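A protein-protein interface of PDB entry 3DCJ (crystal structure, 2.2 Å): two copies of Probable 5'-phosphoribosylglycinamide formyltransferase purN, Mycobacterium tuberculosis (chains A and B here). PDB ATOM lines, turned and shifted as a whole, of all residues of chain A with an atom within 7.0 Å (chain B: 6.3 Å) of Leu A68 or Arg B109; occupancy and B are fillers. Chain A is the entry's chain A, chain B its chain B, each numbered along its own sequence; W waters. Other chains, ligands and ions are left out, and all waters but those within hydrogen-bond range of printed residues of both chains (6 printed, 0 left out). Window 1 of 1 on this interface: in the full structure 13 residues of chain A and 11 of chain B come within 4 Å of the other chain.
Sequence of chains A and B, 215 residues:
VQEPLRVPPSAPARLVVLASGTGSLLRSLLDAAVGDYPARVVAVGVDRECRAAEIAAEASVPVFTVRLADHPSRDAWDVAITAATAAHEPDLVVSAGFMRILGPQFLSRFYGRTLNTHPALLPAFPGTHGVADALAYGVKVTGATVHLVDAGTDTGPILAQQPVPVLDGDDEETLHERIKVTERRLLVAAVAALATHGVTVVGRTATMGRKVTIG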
ATOM      1  N   ASP A  47      -4.862 -28.155  22.887  1.00  0.00           N
ATOM      2  CA  ASP A  47      -5.305 -26.830  23.274  1.00  0.00           C
ATOM      3  C   ASP A  47      -4.747 -26.449  24.631  1.00  0.00           C
ATOM      4  O   ASP A  47      -5.266 -25.571  25.227  1.00  0.00           O
ATOM      5  CB  ASP A  47      -6.841 -26.738  23.283  1.00  0.00           C
ATOM      6  CG  ASP A  47      -7.486 -27.703  24.279  1.00  0.00           C
ATOM      7  OD1 ASP A  47      -6.855 -28.757  24.600  1.00  0.00           O
ATOM      8  OD2 ASP A  47      -8.636 -27.428  24.744  1.00  0.00           O
ATOM      9  N   VAL A  66      -3.296 -24.674  19.875  1.00  0.00           N
ATOM     10  CA  VAL A  66      -4.252 -23.609  19.642  1.00  0.00           C
ATOM     11  C   VAL A  66      -5.149 -23.408  20.887  1.00  0.00           C
ATOM     12  O   VAL A  66      -6.092 -24.201  21.107  1.00  0.00           O
ATOM     13  CB  VAL A  66      -5.125 -23.852  18.369  1.00  0.00           C
ATOM     14  CG1 VAL A  66      -5.910 -22.584  18.029  1.00  0.00           C
ATOM     15  CG2 VAL A  66      -4.299 -24.312  17.178  1.00  0.00           C
ATOM     16  N   ARG A  67      -4.875 -22.369  21.680  1.00  0.00           N
ATOM     17  CA  ARG A  67      -5.575 -22.166  22.960  1.00  0.00           C
ATOM     18  C   ARG A  67      -6.815 -21.282  22.775  1.00  0.00           C
ATOM     19  O   ARG A  67      -6.737 -20.200  22.148  1.00  0.00           O
ATOM     20  CB  ARG A  67      -4.664 -21.510  24.018  1.00  0.00           C
ATOM     21  CG  ARG A  67      -3.495 -22.375  24.588  1.00  0.00           C
ATOM     22  CD  ARG A  67      -2.497 -21.499  25.429  1.00  0.00           C
ATOM     23  NE  ARG A  67      -1.313 -22.336  25.727  1.00  0.00           N
ATOM     24  CZ  ARG A  67      -0.942 -22.803  26.933  1.00  0.00           C
ATOM     25  NH1 ARG A  67      -1.596 -22.467  28.074  1.00  0.00           N
ATOM     26  NH2 ARG A  67       0.132 -23.600  27.004  1.00  0.00           N
ATOM     27  N   LEU A  68      -7.948 -21.715  23.334  1.00  0.00           N
ATOM     28  CA  LEU A  68      -9.177 -20.882  23.325  1.00  0.00           C
ATOM     29  C   LEU A  68      -8.892 -19.445  23.896  1.00  0.00           C
ATOM     30  O   LEU A  68      -9.349 -18.473  23.359  1.00  0.00           O
ATOM     31  CB  LEU A  68     -10.348 -21.585  24.061  1.00  0.00           C
ATOM     32  CG  LEU A  68     -11.736 -20.890  24.087  1.00  0.00           C
ATOM     33  CD1 LEU A  68     -12.260 -20.736  22.654  1.00  0.00           C
ATOM     34  CD2 LEU A  68     -12.789 -21.710  24.947  1.00  0.00           C
ATOM     35  N   ALA A  69      -8.110 -19.334  24.961  1.00  0.00           N
ATOM     36  CA  ALA A  69      -7.778 -18.041  25.530  1.00  0.00           C
ATOM     37  C   ALA A  69      -7.023 -17.085  24.582  1.00  0.00           C
ATOM     38  O   ALA A  69      -6.894 -15.890  24.916  1.00  0.00           O
ATOM     39  CB  ALA A  69      -6.981 -18.226  26.770  1.00  0.00           C
ATOM     40  N   ASP A  70      -6.491 -17.578  23.454  1.00  0.00           N
ATOM     41  CA  ASP A  70      -5.688 -16.712  22.537  1.00  0.00           C
ATOM     42  C   ASP A  70      -6.519 -16.228  21.334  1.00  0.00           C
ATOM     43  O   ASP A  70      -6.009 -15.507  20.482  1.00  0.00           O
ATOM     44  CB  ASP A  70      -4.430 -17.446  21.970  1.00  0.00           C
ATOM     45  CG  ASP A  70      -3.330 -17.686  23.012  1.00  0.00           C
ATOM     46  OD1 ASP A  70      -3.238 -16.943  23.994  1.00  0.00           O
ATOM     47  OD2 ASP A  70      -2.579 -18.662  22.895  1.00  0.00           O
ATOM     48  N   HIS A  71      -7.802 -16.623  21.260  1.00  0.00           N
ATOM     49  CA  HIS A  71      -8.678 -16.186  20.174  1.00  0.00           C
ATOM     50  C   HIS A  71      -9.906 -15.538  20.779  1.00  0.00           C
ATOM     51  O   HIS A  71     -10.200 -15.798  21.936  1.00  0.00           O
ATOM     52  CB  HIS A  71      -8.960 -17.335  19.182  1.00  0.00           C
ATOM     53  CG  HIS A  71      -7.696 -17.883  18.602  1.00  0.00           C
ATOM     54  ND1 HIS A  71      -7.077 -17.324  17.493  1.00  0.00           N
ATOM     55  CD2 HIS A  71      -6.841 -18.818  19.084  1.00  0.00           C
ATOM     56  CE1 HIS A  71      -5.926 -17.948  17.286  1.00  0.00           C
ATOM     57  NE2 HIS A  71      -5.762 -18.862  18.235  1.00  0.00           N
ATOM     58  N   PRO A  72     -10.545 -14.604  20.041  1.00  0.00           N
ATOM     59  CA  PRO A  72     -11.526 -13.738  20.740  1.00  0.00           C
ATOM     60  C   PRO A  72     -12.865 -14.401  21.099  1.00  0.00           C
ATOM     61  O   PRO A  72     -13.586 -13.896  21.986  1.00  0.00           O
ATOM     62  CB  PRO A  72     -11.729 -12.550  19.777  1.00  0.00           C
ATOM     63  CG  PRO A  72     -10.724 -12.758  18.629  1.00  0.00           C
ATOM     64  CD  PRO A  72     -10.277 -14.169  18.646  1.00  0.00           C
ATOM     65  N   SER A  73     -13.165 -15.533  20.463  1.00  0.00           N
ATOM     66  CA  SER A  73     -14.353 -16.321  20.759  1.00  0.00           C
ATOM     67  C   SER A  73     -14.194 -17.776  20.268  1.00  0.00           C
ATOM     68  O   SER A  73     -13.165 -18.137  19.635  1.00  0.00           O
ATOM     69  CB  SER A  73     -15.533 -15.732  19.975  1.00  0.00           C
ATOM     70  OG  SER A  73     -15.196 -15.748  18.580  1.00  0.00           O
ATOM     71  N   ARG A  74     -15.243 -18.573  20.514  1.00  0.00           N
ATOM     72  CA  ARG A  74     -15.349 -19.945  20.023  1.00  0.00           C
ATOM     73  C   ARG A  74     -15.327 -20.037  18.507  1.00  0.00           C
ATOM     74  O   ARG A  74     -14.609 -20.876  17.981  1.00  0.00           O
ATOM     75  CB  ARG A  74     -16.518 -20.735  20.676  1.00  0.00           C
ATOM     76  CG  ARG A  74     -16.264 -20.987  22.247  1.00  0.00           C
ATOM     77  CD  ARG A  74     -16.837 -22.314  22.757  1.00  0.00           C
ATOM     78  NE  ARG A  74     -18.295 -22.211  22.910  1.00  0.00           N
ATOM     79  CZ  ARG A  74     -19.173 -23.200  22.723  1.00  0.00           C
ATOM     80  NH1 ARG A  74     -18.779 -24.433  22.397  1.00  0.00           N
ATOM     81  NH2 ARG A  74     -20.464 -22.941  22.884  1.00  0.00           N
ATOM     82  N   ASP A  75     -16.028 -19.159  17.798  1.00  0.00           N
ATOM     83  CA  ASP A  75     -15.972 -19.141  16.318  1.00  0.00           C
ATOM     84  C   ASP A  75     -14.570 -18.810  15.828  1.00  0.00           C
ATOM     85  O   ASP A  75     -14.080 -19.438  14.888  1.00  0.00           O
ATOM     86  CB  ASP A  75     -17.005 -18.175  15.688  1.00  0.00           C
ATOM     87  CG  ASP A  75     -16.711 -17.824  14.181  1.00  0.00           C
ATOM     88  OD1 ASP A  75     -16.383 -18.691  13.316  1.00  0.00           O
ATOM     89  OD2 ASP A  75     -16.843 -16.627  13.852  1.00  0.00           O
ATOM     90  N   ALA A  76     -13.893 -17.823  16.431  1.00  0.00           N
ATOM     91  CA  ALA A  76     -12.551 -17.562  15.919  1.00  0.00           C
ATOM     92  C   ALA A  76     -11.521 -18.721  16.259  1.00  0.00           C
ATOM     93  O   ALA A  76     -10.571 -18.942  15.515  1.00  0.00           O
ATOM     94  CB  ALA A  76     -12.062 -16.202  16.366  1.00  0.00           C
ATOM     95  N   TRP A  77     -11.755 -19.446  17.365  1.00  0.00           N
ATOM     96  CA  TRP A  77     -10.928 -20.572  17.763  1.00  0.00           C
ATOM     97  C   TRP A  77     -11.174 -21.725  16.749  1.00  0.00           C
ATOM     98  O   TRP A  77     -10.251 -22.466  16.332  1.00  0.00           O
ATOM     99  CB  TRP A  77     -11.269 -21.020  19.211  1.00  0.00           C
ATOM    100  CG  TRP A  77     -10.475 -22.234  19.558  1.00  0.00           C
ATOM    101  CD1 TRP A  77      -9.201 -22.264  20.062  1.00  0.00           C
ATOM    102  CD2 TRP A  77     -10.868 -23.604  19.364  1.00  0.00           C
ATOM    103  NE1 TRP A  77      -8.770 -23.582  20.192  1.00  0.00           N
ATOM    104  CE2 TRP A  77      -9.772 -24.425  19.790  1.00  0.00           C
ATOM    105  CE3 TRP A  77     -12.052 -24.227  18.922  1.00  0.00           C
ATOM    106  CZ2 TRP A  77      -9.807 -25.849  19.739  1.00  0.00           C
ATOM    107  CZ3 TRP A  77     -12.086 -25.662  18.864  1.00  0.00           C
ATOM    108  CH2 TRP A  77     -10.961 -26.435  19.272  1.00  0.00           C
ATOM    109  N   ASP A  78     -12.441 -21.867  16.347  1.00  0.00           N
ATOM    110  CA  ASP A  78     -12.787 -22.876  15.367  1.00  0.00           C
ATOM    111  C   ASP A  78     -11.976 -22.572  14.087  1.00  0.00           C
ATOM    112  O   ASP A  78     -11.328 -23.497  13.487  1.00  0.00           O
ATOM    113  CB  ASP A  78     -14.321 -22.887  15.188  1.00  0.00           C
ATOM    114  CG  ASP A  78     -14.793 -23.705  13.993  1.00  0.00           C
ATOM    115  OD1 ASP A  78     -14.074 -24.671  13.585  1.00  0.00           O
ATOM    116  OD2 ASP A  78     -15.895 -23.339  13.478  1.00  0.00           O
ATOM    117  N   ARG A 100     -12.444 -29.906  23.211  1.00  0.00           N
ATOM    118  CA  ARG A 100     -13.203 -28.857  22.614  1.00  0.00           C
ATOM    119  C   ARG A 100     -14.063 -29.479  21.556  1.00  0.00           C
ATOM    120  O   ARG A 100     -13.636 -30.410  20.876  1.00  0.00           O
ATOM    121  CB  ARG A 100     -12.291 -27.872  21.948  1.00  0.00           C
ATOM    122  CG  ARG A 100     -11.264 -27.288  22.872  1.00  0.00           C
ATOM    123  CD  ARG A 100     -11.788 -26.107  23.618  1.00  0.00           C
ATOM    124  NE  ARG A 100     -10.739 -25.560  24.478  1.00  0.00           N
ATOM    125  CZ  ARG A 100     -10.987 -24.980  25.641  1.00  0.00           C
ATOM    126  NH1 ARG A 100     -12.230 -24.875  26.019  1.00  0.00           N
ATOM    127  NH2 ARG A 100     -10.014 -24.513  26.401  1.00  0.00           N
ATOM    128  N   THR B  82     -12.585  -9.028  30.794  1.00  0.00           N
ATOM    129  CA  THR B  82     -12.535 -10.214  29.924  1.00  0.00           C
ATOM    130  C   THR B  82     -11.118 -10.756  29.720  1.00  0.00           C
ATOM    131  O   THR B  82     -10.902 -11.958  29.764  1.00  0.00           O
ATOM    132  CB  THR B  82     -13.124  -9.868  28.533  1.00  0.00           C
ATOM    133  OG1 THR B  82     -14.434  -9.299  28.699  1.00  0.00           O
ATOM    134  CG2 THR B  82     -13.159 -11.068  27.585  1.00  0.00           C
ATOM    135  N   ALA B  83     -10.165  -9.852  29.479  1.00  0.00           N
ATOM    136  CA  ALA B  83      -8.770 -10.221  29.317  1.00  0.00           C
ATOM    137  C   ALA B  83      -8.167 -10.712  30.637  1.00  0.00           C
ATOM    138  O   ALA B  83      -7.396 -11.677  30.662  1.00  0.00           O
ATOM    139  CB  ALA B  83      -7.917  -8.985  28.708  1.00  0.00           C
ATOM    140  N   THR B  85      -9.709 -12.199  32.987  1.00  0.00           N
ATOM    141  CA  THR B  85     -10.297 -13.529  33.182  1.00  0.00           C
ATOM    142  C   THR B  85      -9.672 -14.588  32.229  1.00  0.00           C
ATOM    143  O   THR B  85      -9.235 -15.654  32.657  1.00  0.00           O
ATOM    144  CB  THR B  85     -11.788 -13.448  32.974  1.00  0.00           C
ATOM    145  OG1 THR B  85     -12.330 -12.515  33.917  1.00  0.00           O
ATOM    146  CG2 THR B  85     -12.457 -14.771  33.203  1.00  0.00           C
ATOM    147  N   ALA B  86      -9.666 -14.282  30.930  1.00  0.00           N
ATOM    148  CA  ALA B  86      -9.105 -15.159  29.911  1.00  0.00           C
ATOM    149  C   ALA B  86      -7.676 -15.573  30.269  1.00  0.00           C
ATOM    150  O   ALA B  86      -7.280 -16.735  29.987  1.00  0.00           O
ATOM    151  CB  ALA B  86      -9.143 -14.480  28.539  1.00  0.00           C
ATOM    152  N   GLU B  89      -7.346 -18.813  31.861  1.00  0.00           N
ATOM    153  CA  GLU B  89      -7.792 -19.937  31.038  1.00  0.00           C
ATOM    154  C   GLU B  89      -8.891 -20.748  31.687  1.00  0.00           C
ATOM    155  O   GLU B  89      -8.750 -21.970  31.884  1.00  0.00           O
ATOM    156  CB  GLU B  89      -6.598 -20.811  30.661  1.00  0.00           C
ATOM    157  CG  GLU B  89      -5.645 -20.085  29.694  1.00  0.00           C
ATOM    158  CD  GLU B  89      -4.619 -21.025  29.062  1.00  0.00           C
ATOM    159  OE1 GLU B  89      -3.585 -21.289  29.690  1.00  0.00           O
ATOM    160  OE2 GLU B  89      -4.855 -21.477  27.941  1.00  0.00           O
ATOM    161  N   PRO B  90     -10.005 -20.077  32.036  1.00  0.00           N
ATOM    162  CA  PRO B  90     -11.043 -20.779  32.805  1.00  0.00           C
ATOM    163  C   PRO B  90     -11.836 -21.737  31.921  1.00  0.00           C
ATOM    164  O   PRO B  90     -11.936 -21.482  30.730  1.00  0.00           O
ATOM    165  CB  PRO B  90     -12.004 -19.626  33.238  1.00  0.00           C
ATOM    166  CG  PRO B  90     -11.902 -18.619  32.167  1.00  0.00           C
ATOM    167  CD  PRO B  90     -10.379 -18.668  31.754  1.00  0.00           C
ATOM    168  N   PRO B 104     -21.027  -7.009  26.575  1.00  0.00           N
ATOM    169  CA  PRO B 104     -20.980  -7.905  25.367  1.00  0.00           C
ATOM    170  C   PRO B 104     -19.577  -8.486  25.048  1.00  0.00           C
ATOM    171  O   PRO B 104     -19.505  -9.601  24.454  1.00  0.00           O
ATOM    172  CB  PRO B 104     -21.466  -7.002  24.208  1.00  0.00           C
ATOM    173  CG  PRO B 104     -21.280  -5.526  24.739  1.00  0.00           C
ATOM    174  CD  PRO B 104     -21.415  -5.601  26.265  1.00  0.00           C
ATOM    175  N   GLN B 105     -18.487  -7.803  25.434  1.00  0.00           N
ATOM    176  CA  GLN B 105     -17.140  -8.368  25.126  1.00  0.00           C
ATOM    177  C   GLN B 105     -16.883  -9.581  25.975  1.00  0.00           C
ATOM    178  O   GLN B 105     -16.411 -10.599  25.466  1.00  0.00           O
ATOM    179  CB  GLN B 105     -15.962  -7.397  25.335  1.00  0.00           C
ATOM    180  CG  GLN B 105     -16.155  -5.942  24.758  1.00  0.00           C
ATOM    181  CD  GLN B 105     -15.953  -5.774  23.211  1.00  0.00           C
ATOM    182  OE1 GLN B 105     -15.708  -6.759  22.463  1.00  0.00           O
ATOM    183  NE2 GLN B 105     -16.044  -4.487  22.739  1.00  0.00           N
ATOM    184  N   PHE B 106     -17.190  -9.477  27.271  1.00  0.00           N
ATOM    185  CA  PHE B 106     -17.096 -10.612  28.173  1.00  0.00           C
ATOM    186  C   PHE B 106     -17.968 -11.761  27.648  1.00  0.00           C
ATOM    187  O   PHE B 106     -17.491 -12.901  27.535  1.00  0.00           O
ATOM    188  CB  PHE B 106     -17.578 -10.252  29.580  1.00  0.00           C
ATOM    189  CG  PHE B 106     -17.212 -11.290  30.605  1.00  0.00           C
ATOM    190  CD1 PHE B 106     -16.020 -11.171  31.324  1.00  0.00           C
ATOM    191  CD2 PHE B 106     -18.061 -12.392  30.839  1.00  0.00           C
ATOM    192  CE1 PHE B 106     -15.651 -12.195  32.291  1.00  0.00           C
ATOM    193  CE2 PHE B 106     -17.730 -13.375  31.761  1.00  0.00           C
ATOM    194  CZ  PHE B 106     -16.496 -13.286  32.472  1.00  0.00           C
ATOM    195  N   LEU B 107     -19.229 -11.471  27.319  1.00  0.00           N
ATOM    196  CA  LEU B 107     -20.124 -12.551  26.844  1.00  0.00           C
ATOM    197  C   LEU B 107     -19.713 -13.155  25.486  1.00  0.00           C
ATOM    198  O   LEU B 107     -19.932 -14.325  25.221  1.00  0.00           O
ATOM    199  CB  LEU B 107     -21.617 -12.150  26.908  1.00  0.00           C
ATOM    200  CG  LEU B 107     -22.003 -11.942  28.397  1.00  0.00           C
ATOM    201  CD1 LEU B 107     -23.360 -11.386  28.502  1.00  0.00           C
ATOM    202  CD2 LEU B 107     -21.849 -13.236  29.312  1.00  0.00           C
ATOM    203  N   SER B 108     -19.067 -12.354  24.653  1.00  0.00           N
ATOM    204  CA  SER B 108     -18.624 -12.864  23.356  1.00  0.00           C
ATOM    205  C   SER B 108     -17.525 -13.904  23.543  1.00  0.00           C
ATOM    206  O   SER B 108     -17.414 -14.830  22.744  1.00  0.00           O
ATOM    207  CB  SER B 108     -18.185 -11.698  22.472  1.00  0.00           C
ATOM    208  OG  SER B 108     -17.192 -12.137  21.583  1.00  0.00           O
ATOM    209  N   ARG B 109     -16.720 -13.778  24.603  1.00  0.00           N
ATOM    210  CA  ARG B 109     -15.766 -14.843  24.964  1.00  0.00           C
ATOM    211  C   ARG B 109     -16.412 -15.980  25.780  1.00  0.00           C
ATOM    212  O   ARG B 109     -16.173 -17.176  25.549  1.00  0.00           O
ATOM    213  CB  ARG B 109     -14.579 -14.267  25.717  1.00  0.00           C
ATOM    214  CG  ARG B 109     -13.528 -15.295  26.179  1.00  0.00           C
ATOM    215  CD  ARG B 109     -12.336 -14.601  26.846  1.00  0.00           C
ATOM    216  NE  ARG B 109     -11.412 -13.977  25.900  1.00  0.00           N
ATOM    217  CZ  ARG B 109     -10.707 -14.657  25.000  1.00  0.00           C
ATOM    218  NH1 ARG B 109      -9.893 -14.023  24.168  1.00  0.00           N
ATOM    219  NH2 ARG B 109     -10.785 -15.974  24.953  1.00  0.00           N
ATOM    220  N   PHE B 110     -17.277 -15.622  26.718  1.00  0.00           N
ATOM    221  CA  PHE B 110     -17.578 -16.602  27.747  1.00  0.00           C
ATOM    222  C   PHE B 110     -19.028 -17.106  27.770  1.00  0.00           C
ATOM    223  O   PHE B 110     -19.351 -17.902  28.621  1.00  0.00           O
ATOM    224  CB  PHE B 110     -17.210 -16.035  29.111  1.00  0.00           C
ATOM    225  CG  PHE B 110     -15.746 -15.935  29.345  1.00  0.00           C
ATOM    226  CD1 PHE B 110     -14.978 -17.061  29.401  1.00  0.00           C
ATOM    227  CD2 PHE B 110     -15.138 -14.710  29.537  1.00  0.00           C
ATOM    228  CE1 PHE B 110     -13.664 -17.008  29.619  1.00  0.00           C
ATOM    229  CE2 PHE B 110     -13.769 -14.653  29.758  1.00  0.00           C
ATOM    230  CZ  PHE B 110     -13.039 -15.817  29.798  1.00  0.00           C
ATOM    231  N   TYR B 111     -19.897 -16.586  26.906  1.00  0.00           N
ATOM    232  CA  TYR B 111     -21.286 -16.998  26.946  1.00  0.00           C
ATOM    233  C   TYR B 111     -21.344 -18.542  26.821  1.00  0.00           C
ATOM    234  O   TYR B 111     -20.616 -19.138  25.974  1.00  0.00           O
ATOM    235  CB  TYR B 111     -22.142 -16.326  25.837  1.00  0.00           C
ATOM    236  CG  TYR B 111     -23.536 -16.927  25.833  1.00  0.00           C
ATOM    237  CD1 TYR B 111     -24.396 -16.684  26.901  1.00  0.00           C
ATOM    238  CD2 TYR B 111     -23.962 -17.810  24.809  1.00  0.00           C
ATOM    239  CE1 TYR B 111     -25.647 -17.223  26.962  1.00  0.00           C
ATOM    240  CE2 TYR B 111     -25.229 -18.394  24.863  1.00  0.00           C
ATOM    241  CZ  TYR B 111     -26.065 -18.096  25.972  1.00  0.00           C
ATOM    242  OH  TYR B 111     -27.329 -18.590  26.114  1.00  0.00           O
ATOM    243  N   ARG B 113     -20.496 -20.546  29.227  1.00  0.00           N
ATOM    244  CA  ARG B 113     -19.569 -21.034  30.247  1.00  0.00           C
ATOM    245  C   ARG B 113     -19.654 -20.156  31.484  1.00  0.00           C
ATOM    246  O   ARG B 113     -18.903 -20.345  32.428  1.00  0.00           O
ATOM    247  CB  ARG B 113     -18.135 -21.071  29.691  1.00  0.00           C
ATOM    248  CG  ARG B 113     -17.944 -22.154  28.660  1.00  0.00           C
ATOM    249  CD  ARG B 113     -16.484 -22.254  28.199  1.00  0.00           C
ATOM    250  NE  ARG B 113     -16.058 -21.033  27.543  1.00  0.00           N
ATOM    251  CZ  ARG B 113     -14.831 -20.506  27.601  1.00  0.00           C
ATOM    252  NH1 ARG B 113     -14.586 -19.372  26.929  1.00  0.00           N
ATOM    253  NH2 ARG B 113     -13.847 -21.095  28.309  1.00  0.00           N
HETATM  254  O   HOH W   1     -17.429 -17.629  22.315  1.00  0.00           O
HETATM  255  O   HOH W   2     -13.345 -24.057  28.384  1.00  0.00           O
HETATM  256  O   HOH W   3      -7.397 -21.661  26.537  1.00  0.00           O
HETATM  257  O   HOH W   4      -8.131 -13.173  21.907  1.00  0.00           O
HETATM  258  O   HOH W   5      -6.601 -13.248  23.957  1.00  0.00           O
HETATM  259  O   HOH W   6      -4.309 -23.961  27.683  1.00  0.00           O
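NH2 of Arg B109 is in hydrogen-bond range of O of Leu A68 (3.3 Å). The guanidinium group of Arg A67 is in salt-bridge range of the side-chain carboxylate of Glu B89 (2.8 Å). The backbone carbonyl oxygen of His A71 lies within hydrogen-bond range of the guanidinium group of Arg B109, at 2.9 Å.
The side-chain hydroxyl (OG) of Ser A73 lies within hydrogen-bond range of the backbone NH (N) of Ala A76, at 3.3 Å. The guanidinium group of Arg B113 is in hydrogen-bond range of the backbone carbonyl oxygen of Pro B90 (3.1 Å). The backbone carbonyl oxygen of Arg B109 lies within hydrogen-bond range of the guanidinium group of Arg B113.
CD2 of Leu A68 touches NH1 of Arg B113, at 3.6 Å. Ala A69 touches Ala B86 (CB to O, 3.6 Å). Glu B89 touches Ala A69 (CG to CB, 3.7 Å). Arg B109 touches Ala A69 (NH1 to O, 3.6 Å). Arg B109 touches Pro A72. O of Ser B108 touches CB of Ser A73, 3.5 Å away.
Leu A68 touches just these residues of chain B: Arg B109 and Arg B113. Printed residues of chain B within 4 Å of Ala A69: Ala B86 (3.6 Å), Glu B89 (3.7 Å) and Arg B109 (3.6 Å). Printed residues of chain A within 4 Å of Ala B86: Ala A69 (3.6 Å). Leu B107 touches none of the printed residues of chain A. The nearest residue of chain B that does not touch Leu A68 is Glu B89 (5.6 Å). The nearest residue of chain A that does not touch Arg B109 is Ser A73 (4.7 Å).
Of the 15 printed residues of chain A, 6 touch a printed residue of chain B. Printed residues of chain A that touch a printed residue of chain B: Arg A67, Leu A68, Ala A69, His A71, Pro A72 and Ser A73. Hydrophobic or aromatic side chains of chain A within 4 Å of the printed part of chain B: Leu A68 and Ala A69. Of the 15 printed residues of chain B, 5 touch a printed residue of chain A. Printed residues of chain B that touch a printed residue of chain A: Ala B86, Glu B89, Ser B108, Arg B109 and Arg B113. Among the printed residues, Asp or Glu carboxylates within 4 Å of a Lys or Arg side-chain nitrogen of the other chain: Arg A67 with Glu B89.
No position is printed for both chains. Of the 9 pairs that touch across the chains among the printed residues, none has its exchanged pair printed and touching as well.
Water W6 lies within hydrogen-bond range of OE2 of Glu B89 (2.6 Å), O of Asp A47 (3.1 Å) and NH1 of Arg A67 (3.1 Å). Water W2 lies within hydrogen-bond range of NH1 of Arg A100 (2.7 Å) and NH2 of Arg B113 (3.0 Å). Water W5 lies within hydrogen-bond range of the backbone carbonyl oxygen (O) of Ala A69 (2.8 Å) and the guanidinium group (NH1) of Arg B109 (3.4 Å). Water W1 lies within hydrogen-bond range of O of Ser B108 (2.8 Å), N of Arg A74 (3.0 Å) and O of Arg B109 (3.5 Å). Water W3 lies within hydrogen-bond range of N of Ala A69, OE2 of Glu B89 and N of Leu A68. Water W4 lies within hydrogen-bond range of NH1 of Arg B109 (3.0 Å), O of His A71 (3.3 Å) and O of Asp A70 (3.5 Å).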
